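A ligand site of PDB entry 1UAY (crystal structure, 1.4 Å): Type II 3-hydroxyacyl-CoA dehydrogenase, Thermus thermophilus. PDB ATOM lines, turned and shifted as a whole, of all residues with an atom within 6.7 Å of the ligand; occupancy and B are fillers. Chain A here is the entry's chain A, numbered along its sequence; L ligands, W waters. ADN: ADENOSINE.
An oxygen (O5') of the ligand sits at hydrogen-bond distance from the backbone carbonyl oxygen (O) of Ala 73 (2.8 Å).
N6 of the ligand sits at hydrogen-bond distance from OD1 of Asp 47 (2.8 Å).
The guanidinium group (NH1) of Arg 35 is in hydrogen-bond range of an oxygen (O2') of the ligand, 2.8 Å away.
N of Val 48 sits at hydrogen-bond distance from N1 of the ligand.
An oxygen (O2') of the ligand sits at hydrogen-bond distance from the side-chain carboxylate (OD1) of Asp 33, 2.6 Å away.
OG of Ser 12 is in hydrogen-bond range of O3' of the ligand.
The backbone NH of Gly 75 lies within hydrogen-bond range of an oxygen (O5') of the ligand (3.3 Å).
The backbone NH (N) of Ala 74 is in hydrogen-bond range of the side-chain hydroxyl (OG1) of Thr 8 (3.2 Å).
The backbone NH of Ala 73 is in hydrogen-bond range of the side-chain hydroxyl of Thr 8 (3.0 Å).
The backbone NH (N) of Val 76 sits at hydrogen-bond distance from the side-chain amide oxygen (OD1) of Asn 101 (2.8 Å).
N of Ala 11 is in hydrogen-bond range of OD2 of Asp 33, 3.0 Å away.
The side-chain carboxylate (OD1) of Asp 47 lies within hydrogen-bond range of the side-chain hydroxyl (OG1) of Thr 49.
O of Gly 46 lies within hydrogen-bond range of N of Leu 34 (3.4 Å).
The backbone NH of Gly 10 is in hydrogen-bond range of the side-chain carboxylate of Asp 33 (3.4 Å).
The backbone NH (N) of Gly 46 is in hydrogen-bond range of the backbone carbonyl oxygen (O) of Asp 33 (3.0 Å).
Gly 9 touches the ligand.
Ala 11 touches the ligand.
Leu 34 touches the ligand (N to N3, 3.6 Å).
Gly 46 touches the ligand.
Ala 74 touches the ligand.
CG1 of Val 76 touches N7 of the ligand, 3.8 Å away.
CG1 of Val 100 touches N7 of the ligand, 3.8 Å away.
Hydrophobic or aromatic side chains that line the ligand: Ala 11, Leu 34, Val 48, Ala 74, Val 76 and Val 100.
Along chain A the residues within 4 Å of the ligand span positions 9 to 100.
Water W2 lies within hydrogen-bond range of an oxygen (O5') of the ligand and the backbone NH of Gly 75.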
ATOM      1  N   THR A   8      -1.891   5.535  -6.826  1.00  0.00           N
ATOM      2  CA  THR A   8      -2.002   5.851  -5.412  1.00  0.00           C
ATOM      3  C   THR A   8      -1.019   6.982  -5.142  1.00  0.00           C
ATOM      4  O   THR A   8       0.048   7.043  -5.759  1.00  0.00           O
ATOM      5  CB  THR A   8      -1.695   4.630  -4.498  1.00  0.00           C
ATOM      6  OG1 THR A   8      -0.298   4.337  -4.510  1.00  0.00           O
ATOM      7  CG2 THR A   8      -2.480   3.412  -4.951  1.00  0.00           C
ATOM      8  N   GLY A   9      -1.380   7.881  -4.241  1.00  0.00           N
ATOM      9  CA  GLY A   9      -0.533   9.028  -3.933  1.00  0.00           C
ATOM     10  C   GLY A   9      -0.638  10.085  -5.013  1.00  0.00           C
ATOM     11  O   GLY A   9       0.209  10.978  -5.107  1.00  0.00           O
ATOM     12  N   GLY A  10      -1.691   9.992  -5.823  1.00  0.00           N
ATOM     13  CA  GLY A  10      -1.885  10.931  -6.921  1.00  0.00           C
ATOM     14  C   GLY A  10      -2.273  12.358  -6.611  1.00  0.00           C
ATOM     15  O   GLY A  10      -2.440  13.159  -7.530  1.00  0.00           O
ATOM     16  N   ALA A  11      -2.413  12.691  -5.332  1.00  0.00           N
ATOM     17  CA  ALA A  11      -2.783  14.064  -4.963  1.00  0.00           C
ATOM     18  C   ALA A  11      -1.604  15.013  -5.096  1.00  0.00           C
ATOM     19  O   ALA A  11      -1.794  16.216  -5.235  1.00  0.00           O
ATOM     20  CB  ALA A  11      -3.317  14.093  -3.531  1.00  0.00           C
ATOM     21  N   SER A  12      -0.382  14.488  -5.069  1.00  0.00           N
ATOM     22  CA  SER A  12       0.771  15.356  -5.175  1.00  0.00           C
ATOM     23  C   SER A  12       2.050  14.652  -5.627  1.00  0.00           C
ATOM     24  O   SER A  12       2.069  13.433  -5.802  1.00  0.00           O
ATOM     25  CB  SER A  12       1.040  16.039  -3.828  1.00  0.00           C
ATOM     26  OG  SER A  12       1.425  15.078  -2.864  1.00  0.00           O
ATOM     27  N   GLY A  13       3.092  15.447  -5.813  1.00  0.00           N
ATOM     28  CA  GLY A  13       4.394  14.939  -6.205  1.00  0.00           C
ATOM     29  C   GLY A  13       4.467  13.953  -7.355  1.00  0.00           C
ATOM     30  O   GLY A  13       3.925  14.188  -8.436  1.00  0.00           O
ATOM     31  N   LEU A  14       5.165  12.844  -7.119  1.00  0.00           N
ATOM     32  CA  LEU A  14       5.359  11.818  -8.145  1.00  0.00           C
ATOM     33  C   LEU A  14       4.064  11.192  -8.634  1.00  0.00           C
ATOM     34  O   LEU A  14       3.857  11.049  -9.845  1.00  0.00           O
ATOM     35  CB  LEU A  14       6.290  10.727  -7.605  1.00  0.00           C
ATOM     36  CG  LEU A  14       7.627  11.219  -7.049  1.00  0.00           C
ATOM     37  CD1 LEU A  14       8.484  10.019  -6.683  1.00  0.00           C
ATOM     38  CD2 LEU A  14       8.339  12.093  -8.074  1.00  0.00           C
ATOM     39  N   GLY A  15       3.189  10.820  -7.707  1.00  0.00           N
ATOM     40  CA  GLY A  15       1.919  10.220  -8.084  1.00  0.00           C
ATOM     41  C   GLY A  15       1.091  11.158  -8.950  1.00  0.00           C
ATOM     42  O   GLY A  15       0.495  10.740  -9.943  1.00  0.00           O
ATOM     43  N   LEU A  32      -6.031   7.309  -5.882  1.00  0.00           N
ATOM     44  CA  LEU A  32      -6.366   6.877  -4.523  1.00  0.00           C
ATOM     45  C   LEU A  32      -5.362   7.635  -3.670  1.00  0.00           C
ATOM     46  O   LEU A  32      -4.150   7.478  -3.814  1.00  0.00           O
ATOM     47  CB  LEU A  32      -6.171   5.372  -4.320  1.00  0.00           C
ATOM     48  CG  LEU A  32      -6.324   4.920  -2.862  1.00  0.00           C
ATOM     49  CD1 LEU A  32      -7.703   5.310  -2.324  1.00  0.00           C
ATOM     50  CD2 LEU A  32      -6.121   3.417  -2.757  1.00  0.00           C
ATOM     51  N   ASP A  33      -5.869   8.477  -2.768  1.00  0.00           N
ATOM     52  CA  ASP A  33      -5.015   9.284  -1.915  1.00  0.00           C
ATOM     53  C   ASP A  33      -5.856   9.733  -0.725  1.00  0.00           C
ATOM     54  O   ASP A  33      -7.078   9.737  -0.793  1.00  0.00           O
ATOM     55  CB  ASP A  33      -4.518  10.496  -2.711  1.00  0.00           C
ATOM     56  CG  ASP A  33      -3.335  11.197  -2.066  1.00  0.00           C
ATOM     57  OD1 ASP A  33      -3.481  11.734  -0.951  1.00  0.00           O
ATOM     58  OD2 ASP A  33      -2.260  11.228  -2.703  1.00  0.00           O
ATOM     59  N   LEU A  34      -5.188  10.096   0.367  1.00  0.00           N
ATOM     60  CA  LEU A  34      -5.893  10.549   1.556  1.00  0.00           C
ATOM     61  C   LEU A  34      -6.570  11.888   1.268  1.00  0.00           C
ATOM     62  O   LEU A  34      -7.528  12.257   1.932  1.00  0.00           O
ATOM     63  CB  LEU A  34      -4.908  10.737   2.719  1.00  0.00           C
ATOM     64  CG  LEU A  34      -4.245   9.473   3.268  1.00  0.00           C
ATOM     65  CD1 LEU A  34      -3.134   9.885   4.228  1.00  0.00           C
ATOM     66  CD2 LEU A  34      -5.269   8.601   3.958  1.00  0.00           C
ATOM     67  N   ARG A  35      -6.046  12.596   0.274  1.00  0.00           N
ATOM     68  CA  ARG A  35      -6.568  13.907  -0.100  1.00  0.00           C
ATOM     69  C   ARG A  35      -7.041  13.928  -1.552  1.00  0.00           C
ATOM     70  O   ARG A  35      -6.620  13.120  -2.367  1.00  0.00           O
ATOM     71  CB  ARG A  35      -5.486  14.964   0.056  1.00  0.00           C
ATOM     72  CG  ARG A  35      -4.759  14.970   1.388  1.00  0.00           C
ATOM     73  CD  ARG A  35      -3.546  15.881   1.318  1.00  0.00           C
ATOM     74  NE  ARG A  35      -2.862  16.027   2.599  1.00  0.00           N
ATOM     75  CZ  ARG A  35      -2.244  15.041   3.244  1.00  0.00           C
ATOM     76  NH1 ARG A  35      -2.223  13.816   2.729  1.00  0.00           N
ATOM     77  NH2 ARG A  35      -1.650  15.271   4.400  1.00  0.00           N
ATOM     78  N   GLY A  46      -8.990   7.732   0.237  1.00  0.00           N
ATOM     79  CA  GLY A  46      -8.827   6.551   1.048  1.00  0.00           C
ATOM     80  C   GLY A  46      -7.380   6.294   1.421  1.00  0.00           C
ATOM     81  O   GLY A  46      -6.477   7.015   1.007  1.00  0.00           O
ATOM     82  N   ASP A  47      -7.179   5.227   2.195  1.00  0.00           N
ATOM     83  CA  ASP A  47      -5.876   4.841   2.721  1.00  0.00           C
ATOM     84  C   ASP A  47      -5.409   3.520   2.091  1.00  0.00           C
ATOM     85  O   ASP A  47      -6.125   2.522   2.149  1.00  0.00           O
ATOM     86  CB  ASP A  47      -6.020   4.683   4.239  1.00  0.00           C
ATOM     87  CG  ASP A  47      -4.689   4.633   4.960  1.00  0.00           C
ATOM     88  OD1 ASP A  47      -3.804   3.890   4.506  1.00  0.00           O
ATOM     89  OD2 ASP A  47      -4.541   5.315   5.993  1.00  0.00           O
ATOM     90  N   VAL A  48      -4.213   3.517   1.509  1.00  0.00           N
ATOM     91  CA  VAL A  48      -3.680   2.308   0.877  1.00  0.00           C
ATOM     92  C   VAL A  48      -3.486   1.137   1.838  1.00  0.00           C
ATOM     93  O   VAL A  48      -3.375  -0.007   1.404  1.00  0.00           O
ATOM     94  CB  VAL A  48      -2.329   2.560   0.159  1.00  0.00           C
ATOM     95  CG1 VAL A  48      -2.531   3.484  -1.040  1.00  0.00           C
ATOM     96  CG2 VAL A  48      -1.318   3.161   1.115  1.00  0.00           C
ATOM     97  N   THR A  49      -3.459   1.421   3.133  1.00  0.00           N
ATOM     98  CA  THR A  49      -3.294   0.362   4.129  1.00  0.00           C
ATOM     99  C   THR A  49      -4.628  -0.315   4.455  1.00  0.00           C
ATOM    100  O   THR A  49      -4.664  -1.335   5.142  1.00  0.00           O
ATOM    101  CB  THR A  49      -2.696   0.893   5.447  1.00  0.00           C
ATOM    102  OG1 THR A  49      -3.629   1.761   6.096  1.00  0.00           O
ATOM    103  CG2 THR A  49      -1.396   1.653   5.178  1.00  0.00           C
ATOM    104  N   ALA A  73       2.405   5.059  -5.686  1.00  0.00           N
ATOM    105  CA  ALA A  73       3.290   6.169  -5.378  1.00  0.00           C
ATOM    106  C   ALA A  73       2.956   6.807  -4.040  1.00  0.00           C
ATOM    107  O   ALA A  73       3.469   7.871  -3.709  1.00  0.00           O
ATOM    108  CB  ALA A  73       3.234   7.206  -6.488  1.00  0.00           C
ATOM    109  N   ALA A  74       2.081   6.155  -3.276  1.00  0.00           N
ATOM    110  CA  ALA A  74       1.693   6.668  -1.973  1.00  0.00           C
ATOM    111  C   ALA A  74       2.770   6.270  -0.982  1.00  0.00           C
ATOM    112  O   ALA A  74       3.272   5.138  -1.020  1.00  0.00           O
ATOM    113  CB  ALA A  74       0.360   6.089  -1.546  1.00  0.00           C
ATOM    114  N   GLY A  75       3.128   7.180  -0.099  1.00  0.00           N
ATOM    115  CA  GLY A  75       4.150   6.863   0.885  1.00  0.00           C
ATOM    116  C   GLY A  75       4.367   7.963   1.889  1.00  0.00           C
ATOM    117  O   GLY A  75       3.834   9.070   1.757  1.00  0.00           O
ATOM    118  N   VAL A  76       5.155   7.646   2.903  1.00  0.00           N
ATOM    119  CA  VAL A  76       5.479   8.609   3.948  1.00  0.00           C
ATOM    120  C   VAL A  76       6.963   8.517   4.239  1.00  0.00           C
ATOM    121  O   VAL A  76       7.613   7.519   3.917  1.00  0.00           O
ATOM    122  CB  VAL A  76       4.697   8.325   5.259  1.00  0.00           C
ATOM    123  CG1 VAL A  76       3.201   8.472   5.013  1.00  0.00           C
ATOM    124  CG2 VAL A  76       5.029   6.938   5.784  1.00  0.00           C
ATOM    125  N   ARG A  96       4.564   2.376  11.500  1.00  0.00           N
ATOM    126  CA  ARG A  96       3.771   3.206  10.610  1.00  0.00           C
ATOM    127  C   ARG A  96       4.402   3.328   9.222  1.00  0.00           C
ATOM    128  O   ARG A  96       3.709   3.220   8.205  1.00  0.00           O
ATOM    129  CB  ARG A  96       3.583   4.605  11.200  1.00  0.00           C
ATOM    130  CG  ARG A  96       2.815   5.563  10.309  1.00  0.00           C
ATOM    131  CD  ARG A  96       1.426   5.023   9.987  1.00  0.00           C
ATOM    132  NE  ARG A  96       0.666   5.926   9.111  1.00  0.00           N
ATOM    133  CZ  ARG A  96      -0.570   5.690   8.678  1.00  0.00           C
ATOM    134  NH1 ARG A  96      -1.196   4.573   9.035  1.00  0.00           N
ATOM    135  NH2 ARG A  96      -1.179   6.556   7.893  1.00  0.00           N
ATOM    136  N   VAL A 100       2.497   1.923   5.748  1.00  0.00           N
ATOM    137  CA  VAL A 100       2.150   2.704   4.564  1.00  0.00           C
ATOM    138  C   VAL A 100       2.968   2.374   3.326  1.00  0.00           C
ATOM    139  O   VAL A 100       2.418   2.079   2.262  1.00  0.00           O
ATOM    140  CB  VAL A 100       2.286   4.223   4.842  1.00  0.00           C
ATOM    141  CG1 VAL A 100       1.905   5.010   3.589  1.00  0.00           C
ATOM    142  CG2 VAL A 100       1.410   4.632   6.024  1.00  0.00           C
ATOM    143  N   ASN A 101       4.297   2.406   3.457  1.00  0.00           N
ATOM    144  CA  ASN A 101       5.190   2.175   2.329  1.00  0.00           C
ATOM    145  C   ASN A 101       5.286   0.747   1.819  1.00  0.00           C
ATOM    146  O   ASN A 101       5.369   0.523   0.610  1.00  0.00           O
ATOM    147  CB  ASN A 101       6.595   2.672   2.657  1.00  0.00           C
ATOM    148  CG  ASN A 101       6.648   4.149   2.920  1.00  0.00           C
ATOM    149  OD1 ASN A 101       5.681   4.871   2.687  1.00  0.00           O
ATOM    150  ND2 ASN A 101       7.800   4.626   3.408  1.00  0.00           N
ATOM    151  N   THR A 183       9.535  14.805  -2.457  1.00  0.00           N
ATOM    152  CA  THR A 183       8.709  13.756  -1.866  1.00  0.00           C
ATOM    153  C   THR A 183       8.730  13.839  -0.341  1.00  0.00           C
ATOM    154  O   THR A 183       9.447  14.662   0.225  1.00  0.00           O
ATOM    155  CB  THR A 183       9.221  12.370  -2.286  1.00  0.00           C
ATOM    156  OG1 THR A 183      10.510  12.143  -1.715  1.00  0.00           O
ATOM    157  CG2 THR A 183       9.315  12.273  -3.802  1.00  0.00           C
ATOM    158  N   PRO A 184       7.953  12.975   0.342  1.00  0.00           N
ATOM    159  CA  PRO A 184       7.930  12.984   1.808  1.00  0.00           C
ATOM    160  C   PRO A 184       9.331  12.895   2.410  1.00  0.00           C
ATOM    161  O   PRO A 184       9.588  13.422   3.497  1.00  0.00           O
ATOM    162  CB  PRO A 184       7.071  11.773   2.143  1.00  0.00           C
ATOM    163  CG  PRO A 184       6.073  11.773   1.039  1.00  0.00           C
ATOM    164  CD  PRO A 184       6.939  12.036  -0.184  1.00  0.00           C
ATOM    165  N   GLN A 187      10.616  16.447   2.122  1.00  0.00           N
ATOM    166  CA  GLN A 187       9.698  17.288   2.882  1.00  0.00           C
ATOM    167  C   GLN A 187       9.873  17.212   4.394  1.00  0.00           C
ATOM    168  O   GLN A 187       9.559  18.164   5.114  1.00  0.00           O
ATOM    169  CB  GLN A 187       8.258  16.930   2.497  1.00  0.00           C
ATOM    170  CG  GLN A 187       7.864  17.390   1.098  1.00  0.00           C
ATOM    171  CD  GLN A 187       6.777  16.539   0.479  1.00  0.00           C
ATOM    172  OE1 GLN A 187       5.932  15.983   1.175  1.00  0.00           O
ATOM    173  NE2 GLN A 187       6.784  16.447  -0.846  1.00  0.00           N
HETATM  174  O5' ADN L   1       3.372   9.942  -1.831  1.00  0.00           O
HETATM  175  C5' ADN L   1       2.808  11.180  -1.388  1.00  0.00           C
HETATM  176  C4' ADN L   1       1.284  11.058  -1.649  1.00  0.00           C
HETATM  177  O4' ADN L   1       1.040   9.948  -0.727  1.00  0.00           O
HETATM  178  C3' ADN L   1       0.649  12.259  -0.922  1.00  0.00           C
HETATM  179  O3' ADN L   1      -0.214  12.852  -1.926  1.00  0.00           O
HETATM  180  C2' ADN L   1      -0.170  11.709   0.259  1.00  0.00           C
HETATM  181  O2' ADN L   1      -1.409  12.349   0.542  1.00  0.00           O
HETATM  182  C1' ADN L   1      -0.191  10.207  -0.090  1.00  0.00           C
HETATM  183  N9  ADN L   1      -0.408   9.259   1.005  1.00  0.00           N
HETATM  184  C8  ADN L   1       0.352   9.146   2.200  1.00  0.00           C
HETATM  185  N7  ADN L   1      -0.027   8.201   3.011  1.00  0.00           N
HETATM  186  C5  ADN L   1      -1.109   7.618   2.343  1.00  0.00           C
HETATM  187  C6  ADN L   1      -2.005   6.512   2.653  1.00  0.00           C
HETATM  188  N6  ADN L   1      -1.907   5.805   3.781  1.00  0.00           N
HETATM  189  N1  ADN L   1      -3.009   6.190   1.736  1.00  0.00           N
HETATM  190  C2  ADN L   1      -3.138   6.904   0.564  1.00  0.00           C
HETATM  191  N3  ADN L   1      -2.349   7.959   0.171  1.00  0.00           N
HETATM  192  C4  ADN L   1      -1.363   8.258   1.107  1.00  0.00           C
HETATM  193  O   HOH W   1       2.779  11.449   2.670  1.00  0.00           O
HETATM  194  O   HOH W   2       5.847   8.738  -1.238  1.00  0.00           O
HETATM  195  O   HOH W   3       3.090  10.679  -4.841  1.00  0.00           O
